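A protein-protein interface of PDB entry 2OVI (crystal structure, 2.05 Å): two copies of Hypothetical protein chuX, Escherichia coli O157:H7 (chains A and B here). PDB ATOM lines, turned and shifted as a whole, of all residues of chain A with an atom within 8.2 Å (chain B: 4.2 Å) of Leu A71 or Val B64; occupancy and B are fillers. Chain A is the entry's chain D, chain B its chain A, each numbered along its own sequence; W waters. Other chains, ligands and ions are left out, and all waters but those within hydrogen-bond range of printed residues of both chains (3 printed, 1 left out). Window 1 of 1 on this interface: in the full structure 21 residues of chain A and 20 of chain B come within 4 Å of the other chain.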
ATOM      1  N   THR A  61      12.774   3.920  -8.960  1.00  0.00           N
ATOM      2  CA  THR A  61      11.501   3.497  -8.416  1.00  0.00           C
ATOM      3  C   THR A  61      10.673   2.861  -9.521  1.00  0.00           C
ATOM      4  O   THR A  61      10.360   3.512 -10.515  1.00  0.00           O
ATOM      5  CB  THR A  61      10.751   4.680  -7.844  1.00  0.00           C
ATOM      6  OG1 THR A  61      11.576   5.302  -6.858  1.00  0.00           O
ATOM      7  CG2 THR A  61       9.397   4.227  -7.238  1.00  0.00           C
ATOM      8  N   THR A  62      10.355   1.574  -9.354  1.00  0.00           N
ATOM      9  CA  THR A  62       9.558   0.863 -10.322  1.00  0.00           C
ATOM     10  C   THR A  62       8.146   0.911  -9.773  1.00  0.00           C
ATOM     11  O   THR A  62       7.915   0.674  -8.590  1.00  0.00           O
ATOM     12  CB  THR A  62      10.007  -0.610 -10.483  1.00  0.00           C
ATOM     13  OG1 THR A  62      11.394  -0.664 -10.813  1.00  0.00           O
ATOM     14  CG2 THR A  62       9.213  -1.264 -11.606  1.00  0.00           C
ATOM     15  N   LEU A  63       7.188   1.176 -10.639  1.00  0.00           N
ATOM     16  CA  LEU A  63       5.819   1.318 -10.190  1.00  0.00           C
ATOM     17  C   LEU A  63       4.800   0.474 -10.953  1.00  0.00           C
ATOM     18  O   LEU A  63       4.858   0.379 -12.175  1.00  0.00           O
ATOM     19  CB  LEU A  63       5.416   2.783 -10.272  1.00  0.00           C
ATOM     20  CG  LEU A  63       4.037   2.876  -9.642  1.00  0.00           C
ATOM     21  CD1 LEU A  63       3.985   4.101  -8.781  1.00  0.00           C
ATOM     22  CD2 LEU A  63       2.958   2.850 -10.693  1.00  0.00           C
ATOM     23  N   VAL A  64       3.908  -0.174 -10.196  1.00  0.00           N
ATOM     24  CA  VAL A  64       2.842  -0.990 -10.783  1.00  0.00           C
ATOM     25  C   VAL A  64       1.574  -0.421 -10.215  1.00  0.00           C
ATOM     26  O   VAL A  64       1.462  -0.238  -8.988  1.00  0.00           O
ATOM     27  CB  VAL A  64       2.909  -2.473 -10.380  1.00  0.00           C
ATOM     28  CG1 VAL A  64       1.968  -3.255 -11.247  1.00  0.00           C
ATOM     29  CG2 VAL A  64       4.263  -2.987 -10.542  1.00  0.00           C
ATOM     30  N   HIS A  65       0.633  -0.108 -11.094  1.00  0.00           N
ATOM     31  CA  HIS A  65      -0.632   0.510 -10.696  1.00  0.00           C
ATOM     32  C   HIS A  65      -1.823  -0.294 -11.206  1.00  0.00           C
ATOM     33  O   HIS A  65      -2.001  -0.466 -12.398  1.00  0.00           O
ATOM     34  CB  HIS A  65      -0.667   1.923 -11.280  1.00  0.00           C
ATOM     35  CG  HIS A  65      -1.841   2.735 -10.847  1.00  0.00           C
ATOM     36  ND1 HIS A  65      -1.727   3.818  -9.998  1.00  0.00           N
ATOM     37  CD2 HIS A  65      -3.163   2.608 -11.115  1.00  0.00           C
ATOM     38  CE1 HIS A  65      -2.928   4.317  -9.757  1.00  0.00           C
ATOM     39  NE2 HIS A  65      -3.816   3.601 -10.420  1.00  0.00           N
ATOM     40  N   THR A  66      -2.664  -0.769 -10.303  1.00  0.00           N
ATOM     41  CA  THR A  66      -3.811  -1.558 -10.710  1.00  0.00           C
ATOM     42  C   THR A  66      -5.064  -0.830 -10.194  1.00  0.00           C
ATOM     43  O   THR A  66      -4.956   0.225  -9.531  1.00  0.00           O
ATOM     44  CB  THR A  66      -3.691  -2.955 -10.071  1.00  0.00           C
ATOM     45  OG1 THR A  66      -4.368  -3.908 -10.871  1.00  0.00           O
ATOM     46  CG2 THR A  66      -4.322  -2.949  -8.699  1.00  0.00           C
ATOM     47  N   ALA A  67      -6.253  -1.365 -10.473  1.00  0.00           N
ATOM     48  CA  ALA A  67      -7.437  -0.706  -9.944  1.00  0.00           C
ATOM     49  C   ALA A  67      -7.466  -0.773  -8.405  1.00  0.00           C
ATOM     50  O   ALA A  67      -8.104   0.067  -7.761  1.00  0.00           O
ATOM     51  CB  ALA A  67      -8.736  -1.360 -10.511  1.00  0.00           C
ATOM     52  N   ASP A  68      -6.754  -1.735  -7.812  1.00  0.00           N
ATOM     53  CA  ASP A  68      -6.824  -1.955  -6.336  1.00  0.00           C
ATOM     54  C   ASP A  68      -5.562  -1.661  -5.569  1.00  0.00           C
ATOM     55  O   ASP A  68      -5.608  -1.503  -4.355  1.00  0.00           O
ATOM     56  CB  ASP A  68      -7.207  -3.421  -6.000  1.00  0.00           C
ATOM     57  CG  ASP A  68      -8.603  -3.842  -6.542  1.00  0.00           C
ATOM     58  OD1 ASP A  68      -8.730  -4.920  -7.204  1.00  0.00           O
ATOM     59  OD2 ASP A  68      -9.560  -3.091  -6.293  1.00  0.00           O
ATOM     60  N   VAL A  69      -4.413  -1.688  -6.240  1.00  0.00           N
ATOM     61  CA  VAL A  69      -3.179  -1.399  -5.522  1.00  0.00           C
ATOM     62  C   VAL A  69      -2.216  -0.520  -6.291  1.00  0.00           C
ATOM     63  O   VAL A  69      -2.231  -0.473  -7.536  1.00  0.00           O
ATOM     64  CB  VAL A  69      -2.380  -2.693  -5.089  1.00  0.00           C
ATOM     65  CG1 VAL A  69      -3.328  -3.805  -4.529  1.00  0.00           C
ATOM     66  CG2 VAL A  69      -1.565  -3.204  -6.239  1.00  0.00           C
ATOM     67  N   ILE A  70      -1.399   0.207  -5.542  1.00  0.00           N
ATOM     68  CA  ILE A  70      -0.337   1.004  -6.165  1.00  0.00           C
ATOM     69  C   ILE A  70       0.912   0.568  -5.408  1.00  0.00           C
ATOM     70  O   ILE A  70       1.043   0.857  -4.213  1.00  0.00           O
ATOM     71  CB  ILE A  70      -0.483   2.530  -5.944  1.00  0.00           C
ATOM     72  CG1 ILE A  70      -1.741   3.076  -6.626  1.00  0.00           C
ATOM     73  CG2 ILE A  70       0.758   3.223  -6.544  1.00  0.00           C
ATOM     74  CD1 ILE A  70      -3.011   2.411  -6.143  1.00  0.00           C
ATOM     75  N   LEU A  71       1.822  -0.118  -6.074  1.00  0.00           N
ATOM     76  CA  LEU A  71       3.015  -0.553  -5.375  1.00  0.00           C
ATOM     77  C   LEU A  71       4.248   0.018  -6.049  1.00  0.00           C
ATOM     78  O   LEU A  71       4.360  -0.021  -7.280  1.00  0.00           O
ATOM     79  CB  LEU A  71       3.106  -2.085  -5.345  1.00  0.00           C
ATOM     80  CG  LEU A  71       2.006  -2.809  -4.554  1.00  0.00           C
ATOM     81  CD1 LEU A  71       2.329  -4.298  -4.560  1.00  0.00           C
ATOM     82  CD2 LEU A  71       1.939  -2.300  -3.095  1.00  0.00           C
ATOM     83  N   GLU A  72       5.163   0.506  -5.225  1.00  0.00           N
ATOM     84  CA  GLU A  72       6.428   1.076  -5.659  1.00  0.00           C
ATOM     85  C   GLU A  72       7.596   0.329  -5.048  1.00  0.00           C
ATOM     86  O   GLU A  72       7.617   0.072  -3.841  1.00  0.00           O
ATOM     87  CB  GLU A  72       6.559   2.533  -5.193  1.00  0.00           C
ATOM     88  CG  GLU A  72       5.794   3.538  -5.975  1.00  0.00           C
ATOM     89  CD  GLU A  72       5.797   4.854  -5.239  1.00  0.00           C
ATOM     90  OE1 GLU A  72       6.891   5.261  -4.801  1.00  0.00           O
ATOM     91  OE2 GLU A  72       4.718   5.459  -5.082  1.00  0.00           O
ATOM     92  N   PHE A  73       8.595   0.051  -5.870  1.00  0.00           N
ATOM     93  CA  PHE A  73       9.790  -0.636  -5.412  1.00  0.00           C
ATOM     94  C   PHE A  73      10.985   0.281  -5.712  1.00  0.00           C
ATOM     95  O   PHE A  73      11.365   0.534  -6.878  1.00  0.00           O
ATOM     96  CB  PHE A  73       9.922  -1.973  -6.119  1.00  0.00           C
ATOM     97  CG  PHE A  73       8.640  -2.783  -6.126  1.00  0.00           C
ATOM     98  CD1 PHE A  73       7.738  -2.681  -7.179  1.00  0.00           C
ATOM     99  CD2 PHE A  73       8.319  -3.635  -5.058  1.00  0.00           C
ATOM    100  CE1 PHE A  73       6.537  -3.422  -7.169  1.00  0.00           C
ATOM    101  CE2 PHE A  73       7.123  -4.377  -5.040  1.00  0.00           C
ATOM    102  CZ  PHE A  73       6.236  -4.272  -6.089  1.00  0.00           C
ATOM    103  N   SER A  74      11.534   0.815  -4.634  1.00  0.00           N
ATOM    104  CA  SER A  74      12.669   1.693  -4.691  1.00  0.00           C
ATOM    105  C   SER A  74      13.916   0.793  -4.647  1.00  0.00           C
ATOM    106  O   SER A  74      13.989  -0.109  -3.823  1.00  0.00           O
ATOM    107  CB  SER A  74      12.600   2.614  -3.473  1.00  0.00           C
ATOM    108  OG  SER A  74      13.679   3.517  -3.453  1.00  0.00           O
ATOM    109  N   MET A  95      13.138  -6.630  -5.072  1.00  0.00           N
ATOM    110  CA  MET A  95      12.211  -6.800  -6.174  1.00  0.00           C
ATOM    111  C   MET A  95      12.625  -7.841  -7.172  1.00  0.00           C
ATOM    112  O   MET A  95      13.783  -7.909  -7.559  1.00  0.00           O
ATOM    113  CB  MET A  95      11.975  -5.512  -6.947  1.00  0.00           C
ATOM    114  CG  MET A  95      10.940  -5.717  -8.092  1.00  0.00           C
ATOM    115  SD  MET A  95      10.510  -4.198  -9.038  1.00  0.00           S
ATOM    116  CE  MET A  95      11.848  -4.247 -10.295  1.00  0.00           C
ATOM    117  N   SER A  96      11.648  -8.626  -7.616  1.00  0.00           N
ATOM    118  CA  SER A  96      11.879  -9.672  -8.594  1.00  0.00           C
ATOM    119  C   SER A  96      10.583  -9.935  -9.328  1.00  0.00           C
ATOM    120  O   SER A  96       9.615  -9.175  -9.198  1.00  0.00           O
ATOM    121  CB  SER A  96      12.355 -10.968  -7.902  1.00  0.00           C
ATOM    122  OG  SER A  96      13.265 -11.679  -8.739  1.00  0.00           O
ATOM    123  N   GLY A  97      10.545 -11.026 -10.069  1.00  0.00           N
ATOM    124  CA  GLY A  97       9.316 -11.333 -10.788  1.00  0.00           C
ATOM    125  C   GLY A  97       9.566 -11.635 -12.251  1.00  0.00           C
ATOM    126  O   GLY A  97      10.687 -11.963 -12.621  1.00  0.00           O
ATOM    127  N   HIS A  98       8.516 -11.511 -13.068  1.00  0.00           N
ATOM    128  CA  HIS A  98       8.542 -11.767 -14.474  1.00  0.00           C
ATOM    129  C   HIS A  98       7.670 -10.738 -15.187  1.00  0.00           C
ATOM    130  O   HIS A  98       6.576 -10.381 -14.734  1.00  0.00           O
ATOM    131  CB  HIS A  98       8.022 -13.181 -14.774  1.00  0.00           C
ATOM    132  CG  HIS A  98       8.548 -14.217 -13.844  1.00  0.00           C
ATOM    133  ND1 HIS A  98       8.184 -14.264 -12.517  1.00  0.00           N
ATOM    134  CD2 HIS A  98       9.538 -15.129 -13.994  1.00  0.00           C
ATOM    135  CE1 HIS A  98       8.939 -15.147 -11.885  1.00  0.00           C
ATOM    136  NE2 HIS A  98       9.769 -15.681 -12.758  1.00  0.00           N
ATOM    137  N   LEU A 133       4.181  -1.104 -16.830  1.00  0.00           N
ATOM    138  CA  LEU A 133       5.208  -0.815 -15.829  1.00  0.00           C
ATOM    139  C   LEU A 133       5.762   0.598 -16.041  1.00  0.00           C
ATOM    140  O   LEU A 133       5.697   1.123 -17.169  1.00  0.00           O
ATOM    141  CB  LEU A 133       6.338  -1.831 -16.000  1.00  0.00           C
ATOM    142  CG  LEU A 133       7.212  -2.055 -14.786  1.00  0.00           C
ATOM    143  CD1 LEU A 133       6.328  -2.628 -13.737  1.00  0.00           C
ATOM    144  CD2 LEU A 133       8.349  -2.991 -15.108  1.00  0.00           C
ATOM    145  N   LYS A 134       6.270   1.215 -14.962  1.00  0.00           N
ATOM    146  CA  LYS A 134       6.863   2.528 -15.035  1.00  0.00           C
ATOM    147  C   LYS A 134       8.093   2.563 -14.177  1.00  0.00           C
ATOM    148  O   LYS A 134       8.131   1.927 -13.123  1.00  0.00           O
ATOM    149  CB  LYS A 134       5.894   3.619 -14.584  1.00  0.00           C
ATOM    150  CG  LYS A 134       4.679   3.753 -15.476  1.00  0.00           C
ATOM    151  CD  LYS A 134       4.132   5.167 -15.495  1.00  0.00           C
ATOM    152  CE  LYS A 134       2.726   5.243 -14.882  1.00  0.00           C
ATOM    153  NZ  LYS A 134       2.016   6.555 -15.138  1.00  0.00           N
ATOM    154  N   PHE A 136      10.771   5.431 -12.482  1.00  0.00           N
ATOM    155  CA  PHE A 136      11.014   6.849 -12.224  1.00  0.00           C
ATOM    156  C   PHE A 136      12.400   6.964 -11.657  1.00  0.00           C
ATOM    157  O   PHE A 136      12.864   6.087 -10.875  1.00  0.00           O
ATOM    158  CB  PHE A 136      10.062   7.434 -11.173  1.00  0.00           C
ATOM    159  CG  PHE A 136       8.635   7.428 -11.589  1.00  0.00           C
ATOM    160  CD1 PHE A 136       7.903   6.239 -11.600  1.00  0.00           C
ATOM    161  CD2 PHE A 136       8.017   8.613 -12.012  1.00  0.00           C
ATOM    162  CE1 PHE A 136       6.564   6.222 -12.028  1.00  0.00           C
ATOM    163  CE2 PHE A 136       6.690   8.612 -12.438  1.00  0.00           C
ATOM    164  CZ  PHE A 136       5.958   7.414 -12.453  1.00  0.00           C
ATOM    165  N   LEU B  63       3.166 -10.192  -3.820  1.00  0.00           N
ATOM    166  CA  LEU B  63       3.087 -10.287  -5.250  1.00  0.00           C
ATOM    167  C   LEU B  63       1.853  -9.634  -5.820  1.00  0.00           C
ATOM    168  O   LEU B  63       0.771  -9.752  -5.235  1.00  0.00           O
ATOM    169  CB  LEU B  63       3.087 -11.779  -5.629  1.00  0.00           C
ATOM    170  CG  LEU B  63       3.029 -12.238  -7.080  1.00  0.00           C
ATOM    171  CD1 LEU B  63       3.611 -13.631  -7.140  1.00  0.00           C
ATOM    172  CD2 LEU B  63       1.600 -12.223  -7.643  1.00  0.00           C
ATOM    173  N   VAL B  64       2.037  -8.937  -6.949  1.00  0.00           N
ATOM    174  CA  VAL B  64       0.937  -8.312  -7.662  1.00  0.00           C
ATOM    175  C   VAL B  64       0.987  -8.981  -9.029  1.00  0.00           C
ATOM    176  O   VAL B  64       2.032  -9.061  -9.629  1.00  0.00           O
ATOM    177  CB  VAL B  64       1.124  -6.770  -7.822  1.00  0.00           C
ATOM    178  CG1 VAL B  64       0.102  -6.195  -8.789  1.00  0.00           C
ATOM    179  CG2 VAL B  64       0.865  -6.116  -6.509  1.00  0.00           C
ATOM    180  N   HIS B  65      -0.153  -9.454  -9.497  1.00  0.00           N
ATOM    181  CA  HIS B  65      -0.249 -10.155 -10.777  1.00  0.00           C
ATOM    182  C   HIS B  65      -1.171  -9.368 -11.692  1.00  0.00           C
ATOM    183  O   HIS B  65      -2.332  -9.092 -11.358  1.00  0.00           O
ATOM    184  CB  HIS B  65      -0.823 -11.548 -10.564  1.00  0.00           C
ATOM    185  CG  HIS B  65      -0.973 -12.347 -11.823  1.00  0.00           C
ATOM    186  ND1 HIS B  65       0.045 -13.125 -12.341  1.00  0.00           N
ATOM    187  CD2 HIS B  65      -2.025 -12.498 -12.669  1.00  0.00           C
ATOM    188  CE1 HIS B  65      -0.373 -13.714 -13.448  1.00  0.00           C
ATOM    189  NE2 HIS B  65      -1.625 -13.349 -13.671  1.00  0.00           N
ATOM    190  N   THR B  66      -0.640  -8.999 -12.848  1.00  0.00           N
ATOM    191  CA  THR B  66      -1.396  -8.244 -13.827  1.00  0.00           C
ATOM    192  C   THR B  66      -1.383  -9.028 -15.148  1.00  0.00           C
ATOM    193  O   THR B  66      -0.725 -10.073 -15.249  1.00  0.00           O
ATOM    194  CB  THR B  66      -0.741  -6.875 -14.020  1.00  0.00           C
ATOM    195  OG1 THR B  66      -1.749  -5.875 -14.064  1.00  0.00           O
ATOM    196  CG2 THR B  66       0.043  -6.831 -15.294  1.00  0.00           C
ATOM    197  N   VAL B  69       2.422  -8.269 -16.040  1.00  0.00           N
ATOM    198  CA  VAL B  69       3.561  -8.428 -15.145  1.00  0.00           C
ATOM    199  C   VAL B  69       3.201  -9.181 -13.875  1.00  0.00           C
ATOM    200  O   VAL B  69       2.028  -9.241 -13.475  1.00  0.00           O
ATOM    201  CB  VAL B  69       4.172  -7.025 -14.713  1.00  0.00           C
ATOM    202  CG1 VAL B  69       4.393  -6.120 -15.951  1.00  0.00           C
ATOM    203  CG2 VAL B  69       3.235  -6.326 -13.769  1.00  0.00           C
ATOM    204  N   ILE B  70       4.227  -9.791 -13.279  1.00  0.00           N
ATOM    205  CA  ILE B  70       4.079 -10.484 -12.025  1.00  0.00           C
ATOM    206  C   ILE B  70       5.280  -9.973 -11.310  1.00  0.00           C
ATOM    207  O   ILE B  70       6.382 -10.386 -11.600  1.00  0.00           O
ATOM    208  CB  ILE B  70       4.188 -12.030 -12.111  1.00  0.00           C
ATOM    209  CG1 ILE B  70       3.111 -12.636 -13.013  1.00  0.00           C
ATOM    210  CG2 ILE B  70       3.954 -12.617 -10.742  1.00  0.00           C
ATOM    211  CD1 ILE B  70       3.333 -12.461 -14.474  1.00  0.00           C
ATOM    212  N   LEU B  71       5.076  -9.073 -10.359  1.00  0.00           N
ATOM    213  CA  LEU B  71       6.170  -8.508  -9.622  1.00  0.00           C
ATOM    214  C   LEU B  71       6.087  -8.894  -8.176  1.00  0.00           C
ATOM    215  O   LEU B  71       5.019  -8.840  -7.536  1.00  0.00           O
ATOM    216  CB  LEU B  71       6.146  -6.982  -9.726  1.00  0.00           C
ATOM    217  CG  LEU B  71       6.633  -6.381 -11.036  1.00  0.00           C
ATOM    218  CD1 LEU B  71       6.876  -4.890 -10.815  1.00  0.00           C
ATOM    219  CD2 LEU B  71       7.939  -7.036 -11.449  1.00  0.00           C
ATOM    220  N   MET B  95       9.918  -1.499  -0.784  1.00  0.00           N
ATOM    221  CA  MET B  95       8.484  -1.500  -1.024  1.00  0.00           C
ATOM    222  C   MET B  95       7.522  -0.550  -0.273  1.00  0.00           C
ATOM    223  O   MET B  95       7.448  -0.541   0.946  1.00  0.00           O
ATOM    224  CB  MET B  95       7.995  -2.929  -0.867  1.00  0.00           C
ATOM    225  CG  MET B  95       6.526  -3.051  -0.909  1.00  0.00           C
ATOM    226  SD  MET B  95       5.946  -4.688  -0.455  1.00  0.00           S
ATOM    227  CE  MET B  95       4.997  -4.838  -1.705  1.00  0.00           C
ATOM    228  N   SER B  96       6.784   0.269  -1.014  1.00  0.00           N
ATOM    229  CA  SER B  96       5.799   1.116  -0.363  1.00  0.00           C
ATOM    230  C   SER B  96       4.605   1.233  -1.323  1.00  0.00           C
ATOM    231  O   SER B  96       4.582   0.549  -2.352  1.00  0.00           O
ATOM    232  CB  SER B  96       6.386   2.503  -0.037  1.00  0.00           C
ATOM    233  OG  SER B  96       6.761   3.181  -1.242  1.00  0.00           O
ATOM    234  N   ILE B  99      -2.972   0.383  -0.856  1.00  0.00           N
ATOM    235  CA  ILE B  99      -3.896  -0.744  -1.154  1.00  0.00           C
ATOM    236  C   ILE B  99      -5.331  -0.237  -0.885  1.00  0.00           C
ATOM    237  O   ILE B  99      -5.614   0.317   0.188  1.00  0.00           O
ATOM    238  CB  ILE B  99      -3.756  -1.974  -0.178  1.00  0.00           C
ATOM    239  CG1 ILE B  99      -2.302  -2.465  -0.052  1.00  0.00           C
ATOM    240  CG2 ILE B  99      -4.717  -3.094  -0.601  1.00  0.00           C
ATOM    241  CD1 ILE B  99      -1.598  -2.683  -1.309  1.00  0.00           C
ATOM    242  N   LEU B 133      -4.052  -8.781  -4.415  1.00  0.00           N
ATOM    243  CA  LEU B 133      -2.655  -8.927  -3.959  1.00  0.00           C
ATOM    244  C   LEU B 133      -2.492 -10.322  -3.364  1.00  0.00           C
ATOM    245  O   LEU B 133      -3.473 -10.929  -2.935  1.00  0.00           O
ATOM    246  CB  LEU B 133      -2.422  -7.894  -2.810  1.00  0.00           C
ATOM    247  CG  LEU B 133      -0.986  -7.641  -2.330  1.00  0.00           C
ATOM    248  CD1 LEU B 133      -0.240  -6.984  -3.489  1.00  0.00           C
ATOM    249  CD2 LEU B 133      -0.955  -6.736  -1.068  1.00  0.00           C
HETATM  250  O   HOH W   1      -4.875  -6.135 -12.788  1.00  0.00           O
HETATM  251  O   HOH W   2       9.398   2.577  -2.312  1.00  0.00           O
HETATM  252  O   HOH W   3      -4.194  -3.867 -14.195  1.00  0.00           O
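O of Leu B71 lies within hydrogen-bond range of N of Val B64 (3.0 Å). The backbone carbonyl oxygen of Phe A73 sits at hydrogen-bond distance from the backbone NH of Thr A62 (2.9 Å). The backbone NH (N) of Leu A71 lies within hydrogen-bond range of the backbone carbonyl oxygen (O) of Val A64 (2.9 Å).
Among the printed residues, merely in contact across the chains: Leu A71 with Val B64, Gly A97 with Ile B70, Val A64 with Leu B71, Glu A72 with Met B95, Ser A96 with Leu B71, Leu A71 with Ser B96, His A98 with Val B69, Asp A68 with Ile B99, Leu A133 with Leu B71, Val A69 with Val B64, Val A69 with Ile B99, Leu A71 with Leu B133, Leu A71 with Met B95, Phe A73 with Leu B71, Leu A71 with Ile B99 and Phe A73 with Met B95.
Of the printed residues of chain B, Leu A71 touches Val B64, Met B95, Ser B96, Ile B99 and Leu B133. Printed residues of chain B within 4 Å of Phe A73: Leu B71 (3.9 Å) and Met B95 (3.98 Å). Printed residues of chain B within 4 Å of His A98: Val B69 (3.6 Å) and Ile B70 (2.8 Å). Val B64 touches just these residues of chain A: Val A69 (3.8 Å) and Leu A71 (3.0 Å). Of the printed residues of chain A, Val B69 touches His A98. Printed residues of chain A within 4 Å of Ile B99: Asp A68 (3.7 Å), Val A69 (3.8 Å) and Leu A71 (3.98 Å). Of the printed residues of chain A, Leu B133 touches Leu A71. The nearest printed residue of chain B that does not touch His A98 is Leu B71 (4.8 Å).
Water W2 bridges the side-chain hydroxyl (OG) of Ser B96 and the backbone carbonyl oxygen (O) of Glu A72. Water W1 bridges the side-chain hydroxyl of Thr A66 (3.0 Å) and the side-chain hydroxyl of Thr B66 (3.4 Å). Water W3 lies within hydrogen-bond range of OG1 of Thr B66 (3.2 Å) and OG1 of Thr A66 (3.3 Å).
The backbone NH of His A98 lies within hydrogen-bond range of the backbone carbonyl oxygen of Ile B70 (2.8 Å). O of Ser B96 is in hydrogen-bond range of N of Glu A72 (2.9 Å).
Hydrophobic or aromatic side chains of chain A within 4 Å of the printed part of chain B: Val A64, Val A69, Leu A71, Phe A73 and Leu A133. Printed residues of chain B that touch a printed residue of chain A: Val B64, Val B69, Ile B70, Leu B71, Met B95, Ser B96, Ile B99 and Leu B133. Hydrophobic or aromatic side chains of chain B within 4 Å of the printed part of chain A: Val B64, Ile B70, Leu B71, Met B95, Ile B99 and Leu B133. Among the printed residues, no Asp or Glu carboxylate lies within 4 Å of a Lys or Arg side-chain nitrogen of the other chain.
Val A64 touches Leu B71, and with the chains exchanged Leu A71 touches Val B64. Val A69 touches Val B64, but with the chains exchanged Val A64 does not touch Val B69 (4.2 Å). Leu A71 touches Met B95, but with the chains exchanged Met A95 does not touch Leu B71 (4.1 Å). Leu A71 touches Leu B133, and with the chains exchanged Leu A133 touches Leu B71. Of the 18 pairs that touch across the chains among the printed residues, 6 have their exchanged pair printed and touching as well.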
